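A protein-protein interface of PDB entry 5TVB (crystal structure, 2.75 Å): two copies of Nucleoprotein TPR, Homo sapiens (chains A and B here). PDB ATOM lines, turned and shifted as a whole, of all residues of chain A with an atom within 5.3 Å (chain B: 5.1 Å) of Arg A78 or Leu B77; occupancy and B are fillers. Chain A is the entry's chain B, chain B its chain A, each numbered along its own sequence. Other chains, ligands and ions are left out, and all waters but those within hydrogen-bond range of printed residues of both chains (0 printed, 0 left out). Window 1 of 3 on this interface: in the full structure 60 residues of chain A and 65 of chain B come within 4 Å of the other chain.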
ATOM      1  N   THR A  71     -28.221 -17.439   2.137  1.00  0.00           N
ATOM      2  CA  THR A  71     -29.367 -16.591   1.810  1.00  0.00           C
ATOM      3  C   THR A  71     -29.256 -15.232   2.447  1.00  0.00           C
ATOM      4  O   THR A  71     -29.504 -14.206   1.812  1.00  0.00           O
ATOM      5  CB  THR A  71     -30.697 -17.257   2.201  1.00  0.00           C
ATOM      6  OG1 THR A  71     -30.781 -18.548   1.582  1.00  0.00           O
ATOM      7  CG2 THR A  71     -31.864 -16.411   1.721  1.00  0.00           C
ATOM      8  N   GLU A  73     -26.457 -13.840   3.429  1.00  0.00           N
ATOM      9  CA  GLU A  73     -25.318 -13.137   2.847  1.00  0.00           C
ATOM     10  C   GLU A  73     -25.642 -12.633   1.441  1.00  0.00           C
ATOM     11  O   GLU A  73     -25.178 -11.569   1.031  1.00  0.00           O
ATOM     12  CB  GLU A  73     -24.079 -14.040   2.821  1.00  0.00           C
ATOM     13  CG  GLU A  73     -22.817 -13.368   2.283  1.00  0.00           C
ATOM     14  CD  GLU A  73     -22.312 -12.242   3.173  1.00  0.00           C
ATOM     15  OE1 GLU A  73     -22.772 -12.131   4.330  1.00  0.00           O
ATOM     16  OE2 GLU A  73     -21.450 -11.463   2.713  1.00  0.00           O
ATOM     17  N   CYS A  74     -26.438 -13.407   0.707  1.00  0.00           N
ATOM     18  CA  CYS A  74     -26.875 -13.014  -0.630  1.00  0.00           C
ATOM     19  C   CYS A  74     -27.782 -11.790  -0.593  1.00  0.00           C
ATOM     20  O   CYS A  74     -27.556 -10.821  -1.316  1.00  0.00           O
ATOM     21  CB  CYS A  74     -27.597 -14.174  -1.318  1.00  0.00           C
ATOM     22  SG  CYS A  74     -28.104 -13.845  -3.021  1.00  0.00           S
ATOM     23  N   GLN A  75     -28.810 -11.847   0.251  1.00  0.00           N
ATOM     24  CA  GLN A  75     -29.725 -10.724   0.442  1.00  0.00           C
ATOM     25  C   GLN A  75     -28.989  -9.456   0.862  1.00  0.00           C
ATOM     26  O   GLN A  75     -29.269  -8.370   0.352  1.00  0.00           O
ATOM     27  CB  GLN A  75     -30.792 -11.070   1.482  1.00  0.00           C
ATOM     28  CG  GLN A  75     -31.806 -12.102   1.018  1.00  0.00           C
ATOM     29  CD  GLN A  75     -32.494 -12.802   2.175  1.00  0.00           C
ATOM     30  OE1 GLN A  75     -32.120 -12.622   3.335  1.00  0.00           O
ATOM     31  NE2 GLN A  75     -33.510 -13.599   1.866  1.00  0.00           N
ATOM     32  N   SER A  76     -28.056  -9.606   1.798  1.00  0.00           N
ATOM     33  CA  SER A  76     -27.248  -8.492   2.278  1.00  0.00           C
ATOM     34  C   SER A  76     -26.536  -7.788   1.127  1.00  0.00           C
ATOM     35  O   SER A  76     -26.455  -6.564   1.096  1.00  0.00           O
ATOM     36  CB  SER A  76     -26.227  -8.978   3.308  1.00  0.00           C
ATOM     37  OG  SER A  76     -25.267  -7.976   3.594  1.00  0.00           O
ATOM     38  N   LEU A  77     -26.027  -8.572   0.182  1.00  0.00           N
ATOM     39  CA  LEU A  77     -25.352  -8.029  -0.992  1.00  0.00           C
ATOM     40  C   LEU A  77     -26.330  -7.437  -2.006  1.00  0.00           C
ATOM     41  O   LEU A  77     -26.122  -6.333  -2.509  1.00  0.00           O
ATOM     42  CB  LEU A  77     -24.497  -9.108  -1.659  1.00  0.00           C
ATOM     43  CG  LEU A  77     -23.259  -9.539  -0.874  1.00  0.00           C
ATOM     44  CD1 LEU A  77     -22.507 -10.629  -1.615  1.00  0.00           C
ATOM     45  CD2 LEU A  77     -22.359  -8.341  -0.609  1.00  0.00           C
ATOM     46  N   ARG A  78     -27.386  -8.188  -2.307  1.00  0.00           N
ATOM     47  CA  ARG A  78     -28.382  -7.791  -3.302  1.00  0.00           C
ATOM     48  C   ARG A  78     -29.008  -6.432  -2.999  1.00  0.00           C
ATOM     49  O   ARG A  78     -29.294  -5.651  -3.909  1.00  0.00           O
ATOM     50  CB  ARG A  78     -29.468  -8.862  -3.403  1.00  0.00           C
ATOM     51  CG  ARG A  78     -30.368  -8.740  -4.618  1.00  0.00           C
ATOM     52  CD  ARG A  78     -30.997 -10.084  -4.935  1.00  0.00           C
ATOM     53  NE  ARG A  78     -31.431 -10.767  -3.720  1.00  0.00           N
ATOM     54  CZ  ARG A  78     -31.315 -12.075  -3.514  1.00  0.00           C
ATOM     55  NH1 ARG A  78     -30.776 -12.851  -4.446  1.00  0.00           N
ATOM     56  NH2 ARG A  78     -31.735 -12.609  -2.375  1.00  0.00           N
ATOM     57  N   LEU A  79     -29.229  -6.160  -1.717  1.00  0.00           N
ATOM     58  CA  LEU A  79     -29.709  -4.853  -1.280  1.00  0.00           C
ATOM     59  C   LEU A  79     -28.661  -3.782  -1.560  1.00  0.00           C
ATOM     60  O   LEU A  79     -28.976  -2.713  -2.086  1.00  0.00           O
ATOM     61  CB  LEU A  79     -30.067  -4.867   0.207  1.00  0.00           C
ATOM     62  CG  LEU A  79     -31.298  -5.679   0.614  1.00  0.00           C
ATOM     63  CD1 LEU A  79     -31.594  -5.492   2.093  1.00  0.00           C
ATOM     64  CD2 LEU A  79     -32.501  -5.291  -0.228  1.00  0.00           C
ATOM     65  N   GLU A  80     -27.413  -4.075  -1.202  1.00  0.00           N
ATOM     66  CA  GLU A  80     -26.315  -3.134  -1.393  1.00  0.00           C
ATOM     67  C   GLU A  80     -26.155  -2.785  -2.865  1.00  0.00           C
ATOM     68  O   GLU A  80     -25.923  -1.625  -3.211  1.00  0.00           O
ATOM     69  CB  GLU A  80     -25.005  -3.711  -0.857  1.00  0.00           C
ATOM     70  CG  GLU A  80     -24.994  -3.957   0.637  1.00  0.00           C
ATOM     71  CD  GLU A  80     -23.709  -4.605   1.109  1.00  0.00           C
ATOM     72  OE1 GLU A  80     -22.782  -4.758   0.284  1.00  0.00           O
ATOM     73  OE2 GLU A  80     -23.624  -4.960   2.304  1.00  0.00           O
ATOM     74  N   LEU A  81     -26.288  -3.793  -3.722  1.00  0.00           N
ATOM     75  CA  LEU A  81     -26.265  -3.581  -5.164  1.00  0.00           C
ATOM     76  C   LEU A  81     -27.268  -2.497  -5.536  1.00  0.00           C
ATOM     77  O   LEU A  81     -26.949  -1.568  -6.274  1.00  0.00           O
ATOM     78  CB  LEU A  81     -26.581  -4.875  -5.913  1.00  0.00           C
ATOM     79  CG  LEU A  81     -26.415  -4.827  -7.434  1.00  0.00           C
ATOM     80  CD1 LEU A  81     -24.943  -4.880  -7.807  1.00  0.00           C
ATOM     81  CD2 LEU A  81     -27.186  -5.956  -8.102  1.00  0.00           C
ATOM     82  N   GLU A  82     -28.478  -2.623  -4.999  1.00  0.00           N
ATOM     83  CA  GLU A  82     -29.551  -1.671  -5.258  1.00  0.00           C
ATOM     84  C   GLU A  82     -29.208  -0.299  -4.691  1.00  0.00           C
ATOM     85  O   GLU A  82     -29.460   0.728  -5.320  1.00  0.00           O
ATOM     86  CB  GLU A  82     -30.859  -2.153  -4.633  1.00  0.00           C
ATOM     87  CG  GLU A  82     -32.072  -1.322  -5.013  1.00  0.00           C
ATOM     88  CD  GLU A  82     -33.360  -1.880  -4.440  1.00  0.00           C
ATOM     89  OE1 GLU A  82     -33.344  -3.026  -3.940  1.00  0.00           O
ATOM     90  OE2 GLU A  82     -34.400  -1.192  -4.531  1.00  0.00           O
ATOM     91  N   GLU B  73     -24.866 -17.260  -6.962  1.00  0.00           N
ATOM     92  CA  GLU B  73     -25.557 -15.978  -7.003  1.00  0.00           C
ATOM     93  C   GLU B  73     -24.858 -14.926  -6.148  1.00  0.00           C
ATOM     94  O   GLU B  73     -24.865 -13.742  -6.484  1.00  0.00           O
ATOM     95  CB  GLU B  73     -27.010 -16.149  -6.553  1.00  0.00           C
ATOM     96  CG  GLU B  73     -27.842 -14.874  -6.578  1.00  0.00           C
ATOM     97  CD  GLU B  73     -28.054 -14.319  -7.976  1.00  0.00           C
ATOM     98  OE1 GLU B  73     -27.775 -15.035  -8.963  1.00  0.00           O
ATOM     99  OE2 GLU B  73     -28.509 -13.160  -8.086  1.00  0.00           O
ATOM    100  N   CYS B  74     -24.255 -15.359  -5.045  1.00  0.00           N
ATOM    101  CA  CYS B  74     -23.475 -14.453  -4.209  1.00  0.00           C
ATOM    102  C   CYS B  74     -22.286 -13.938  -5.006  1.00  0.00           C
ATOM    103  O   CYS B  74     -22.017 -12.738  -5.042  1.00  0.00           O
ATOM    104  CB  CYS B  74     -22.997 -15.149  -2.935  1.00  0.00           C
ATOM    105  SG  CYS B  74     -24.240 -15.262  -1.635  1.00  0.00           S
ATOM    106  N   GLN B  75     -21.580 -14.872  -5.635  1.00  0.00           N
ATOM    107  CA  GLN B  75     -20.465 -14.561  -6.517  1.00  0.00           C
ATOM    108  C   GLN B  75     -20.894 -13.596  -7.622  1.00  0.00           C
ATOM    109  O   GLN B  75     -20.189 -12.633  -7.926  1.00  0.00           O
ATOM    110  CB  GLN B  75     -19.906 -15.850  -7.120  1.00  0.00           C
ATOM    111  CG  GLN B  75     -19.206 -16.749  -6.111  1.00  0.00           C
ATOM    112  CD  GLN B  75     -19.164 -18.200  -6.550  1.00  0.00           C
ATOM    113  OE1 GLN B  75     -19.779 -18.577  -7.548  1.00  0.00           O
ATOM    114  NE2 GLN B  75     -18.439 -19.025  -5.802  1.00  0.00           N
ATOM    115  N   SER B  76     -22.053 -13.869  -8.217  1.00  0.00           N
ATOM    116  CA  SER B  76     -22.619 -13.014  -9.258  1.00  0.00           C
ATOM    117  C   SER B  76     -22.791 -11.575  -8.783  1.00  0.00           C
ATOM    118  O   SER B  76     -22.551 -10.630  -9.535  1.00  0.00           O
ATOM    119  CB  SER B  76     -23.966 -13.568  -9.732  1.00  0.00           C
ATOM    120  OG  SER B  76     -23.796 -14.786 -10.435  1.00  0.00           O
ATOM    121  N   LEU B  77     -23.205 -11.416  -7.530  1.00  0.00           N
ATOM    122  CA  LEU B  77     -23.391 -10.092  -6.952  1.00  0.00           C
ATOM    123  C   LEU B  77     -22.049  -9.427  -6.682  1.00  0.00           C
ATOM    124  O   LEU B  77     -21.842  -8.273  -7.056  1.00  0.00           O
ATOM    125  CB  LEU B  77     -24.203 -10.177  -5.658  1.00  0.00           C
ATOM    126  CG  LEU B  77     -25.683 -10.554  -5.775  1.00  0.00           C
ATOM    127  CD1 LEU B  77     -26.320 -10.636  -4.399  1.00  0.00           C
ATOM    128  CD2 LEU B  77     -26.434  -9.564  -6.656  1.00  0.00           C
ATOM    129  N   ARG B  78     -21.140 -10.160  -6.043  1.00  0.00           N
ATOM    130  CA  ARG B  78     -19.823  -9.630  -5.691  1.00  0.00           C
ATOM    131  C   ARG B  78     -19.076  -9.109  -6.913  1.00  0.00           C
ATOM    132  O   ARG B  78     -18.388  -8.090  -6.839  1.00  0.00           O
ATOM    133  CB  ARG B  78     -18.983 -10.696  -4.986  1.00  0.00           C
ATOM    134  CG  ARG B  78     -19.522 -11.110  -3.628  1.00  0.00           C
ATOM    135  CD  ARG B  78     -18.513 -11.949  -2.861  1.00  0.00           C
ATOM    136  NE  ARG B  78     -19.071 -12.461  -1.613  1.00  0.00           N
ATOM    137  CZ  ARG B  78     -19.625 -13.661  -1.481  1.00  0.00           C
ATOM    138  NH1 ARG B  78     -19.693 -14.479  -2.523  1.00  0.00           N
ATOM    139  NH2 ARG B  78     -20.109 -14.045  -0.308  1.00  0.00           N
ATOM    140  N   LEU B  79     -19.220  -9.806  -8.035  1.00  0.00           N
ATOM    141  CA  LEU B  79     -18.635  -9.355  -9.290  1.00  0.00           C
ATOM    142  C   LEU B  79     -19.269  -8.048  -9.744  1.00  0.00           C
ATOM    143  O   LEU B  79     -18.574  -7.076 -10.040  1.00  0.00           O
ATOM    144  CB  LEU B  79     -18.808 -10.419 -10.373  1.00  0.00           C
ATOM    145  CG  LEU B  79     -18.627  -9.944 -11.816  1.00  0.00           C
ATOM    146  CD1 LEU B  79     -17.153  -9.839 -12.179  1.00  0.00           C
ATOM    147  CD2 LEU B  79     -19.367 -10.858 -12.781  1.00  0.00           C
ATOM    148  N   GLU B  80     -20.597  -8.033  -9.791  1.00  0.00           N
ATOM    149  CA  GLU B  80     -21.341  -6.852 -10.206  1.00  0.00           C
ATOM    150  C   GLU B  80     -21.133  -5.703  -9.224  1.00  0.00           C
ATOM    151  O   GLU B  80     -21.005  -4.546  -9.627  1.00  0.00           O
ATOM    152  CB  GLU B  80     -22.830  -7.175 -10.343  1.00  0.00           C
ATOM    153  CG  GLU B  80     -23.645  -6.077 -11.010  1.00  0.00           C
ATOM    154  CD  GLU B  80     -23.157  -5.746 -12.410  1.00  0.00           C
ATOM    155  OE1 GLU B  80     -22.579  -6.633 -13.074  1.00  0.00           O
ATOM    156  OE2 GLU B  80     -23.352  -4.593 -12.848  1.00  0.00           O
ATOM    157  N   LEU B  81     -21.124  -6.036  -7.938  1.00  0.00           N
ATOM    158  CA  LEU B  81     -20.848  -5.072  -6.879  1.00  0.00           C
ATOM    159  C   LEU B  81     -19.528  -4.346  -7.103  1.00  0.00           C
ATOM    160  O   LEU B  81     -19.465  -3.122  -7.040  1.00  0.00           O
ATOM    161  CB  LEU B  81     -20.824  -5.768  -5.518  1.00  0.00           C
ATOM    162  CG  LEU B  81     -20.739  -4.887  -4.271  1.00  0.00           C
ATOM    163  CD1 LEU B  81     -22.091  -4.257  -3.972  1.00  0.00           C
ATOM    164  CD2 LEU B  81     -20.234  -5.683  -3.078  1.00  0.00           C
ATOM    165  N   GLU B  82     -18.479  -5.115  -7.373  1.00  0.00           N
ATOM    166  CA  GLU B  82     -17.142  -4.563  -7.559  1.00  0.00           C
ATOM    167  C   GLU B  82     -17.027  -3.668  -8.794  1.00  0.00           C
ATOM    168  O   GLU B  82     -16.383  -2.621  -8.741  1.00  0.00           O
ATOM    169  CB  GLU B  82     -16.122  -5.702  -7.605  1.00  0.00           C
ATOM    170  CG  GLU B  82     -14.672  -5.264  -7.707  1.00  0.00           C
ATOM    171  CD  GLU B  82     -13.708  -6.403  -7.428  1.00  0.00           C
ATOM    172  OE1 GLU B  82     -14.109  -7.364  -6.737  1.00  0.00           O
ATOM    173  OE2 GLU B  82     -12.570  -6.364  -7.940  1.00  0.00           O
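N of Cys A74 sits close to SG of Cys B74, 3.7 Å away.
SG of Cys A74 is in hydrogen-bond range of NH1 of Arg A78, at 3.2 Å.
Arg B78 touches Glu A73. Glu B73 touches Cys A74 (CG to SG, 3.7 Å). Leu B77 touches Cys A74 (CD1 to O, 3.3 Å). Leu B77 touches Leu A77. CD1 of Leu A77 touches CG of Arg B78, 3.6 Å away. Leu B77 touches Arg A78. CD2 of Leu B77 touches CD2 of Leu A81, 3.96 Å away. CD1 of Leu A81 touches CG of Glu B80 (3.7 Å). Leu B81 touches Leu A81.
Printed residues of chain B within 4 Å of Cys A74: Glu B73, Cys B74 and Leu B77. Arg A78 touches just one residue of chain B: Leu B77. Of the printed residues of chain B, Leu A81 touches Leu B77, Glu B80 and Leu B81. Leu B77 touches four residues of chain A. Of the printed residues of chain A, Arg B78 touches Glu A73 (3.8 Å) and Leu A77 (3.6 Å). Leu B79 touches none of the printed residues of chain A. Of the printed residues of chain A, Glu B80 touches Leu A81 (3.7 Å). Of the printed residues of chain A, Leu B81 touches Leu A81 (3.99 Å). The nearest printed residue of chain A that does not touch Leu B77 is Gln A75 (5.4 Å). The nearest printed residue of chain B that does not touch Leu A77 is Cys B74 (4.1 Å).
Of the 10 printed residues of chain B, 6 touch a printed residue of chain A. Hydrophobic or aromatic side chains of chain B within 4 Å of the printed part of chain A: Leu B77. Hydrophobic or aromatic side chains of chain A within 4 Å of the printed part of chain B: Leu A77 and Leu A81. Among the printed residues, 10 pairs touch across the chains. Among the printed residues, no Asp or Glu carboxylate lies within 4 Å of a Lys or Arg side-chain nitrogen of the other chain.
Leu B77 touches its own counterpart, Leu A77. Leu A77 touches Arg B78, and with the chains exchanged Arg A78 touches Leu B77. Leu A81 touches Leu B77, but with the chains exchanged Leu A77 does not touch Leu B81 (4.2 Å). Leu A81 touches Glu B80, but with the chains exchanged Glu A80 does not touch Leu B81 (4.3 Å). Positions printed for both chains: 73, 74, 75, 76, 77, 78, 79, 80, 81 and 82.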
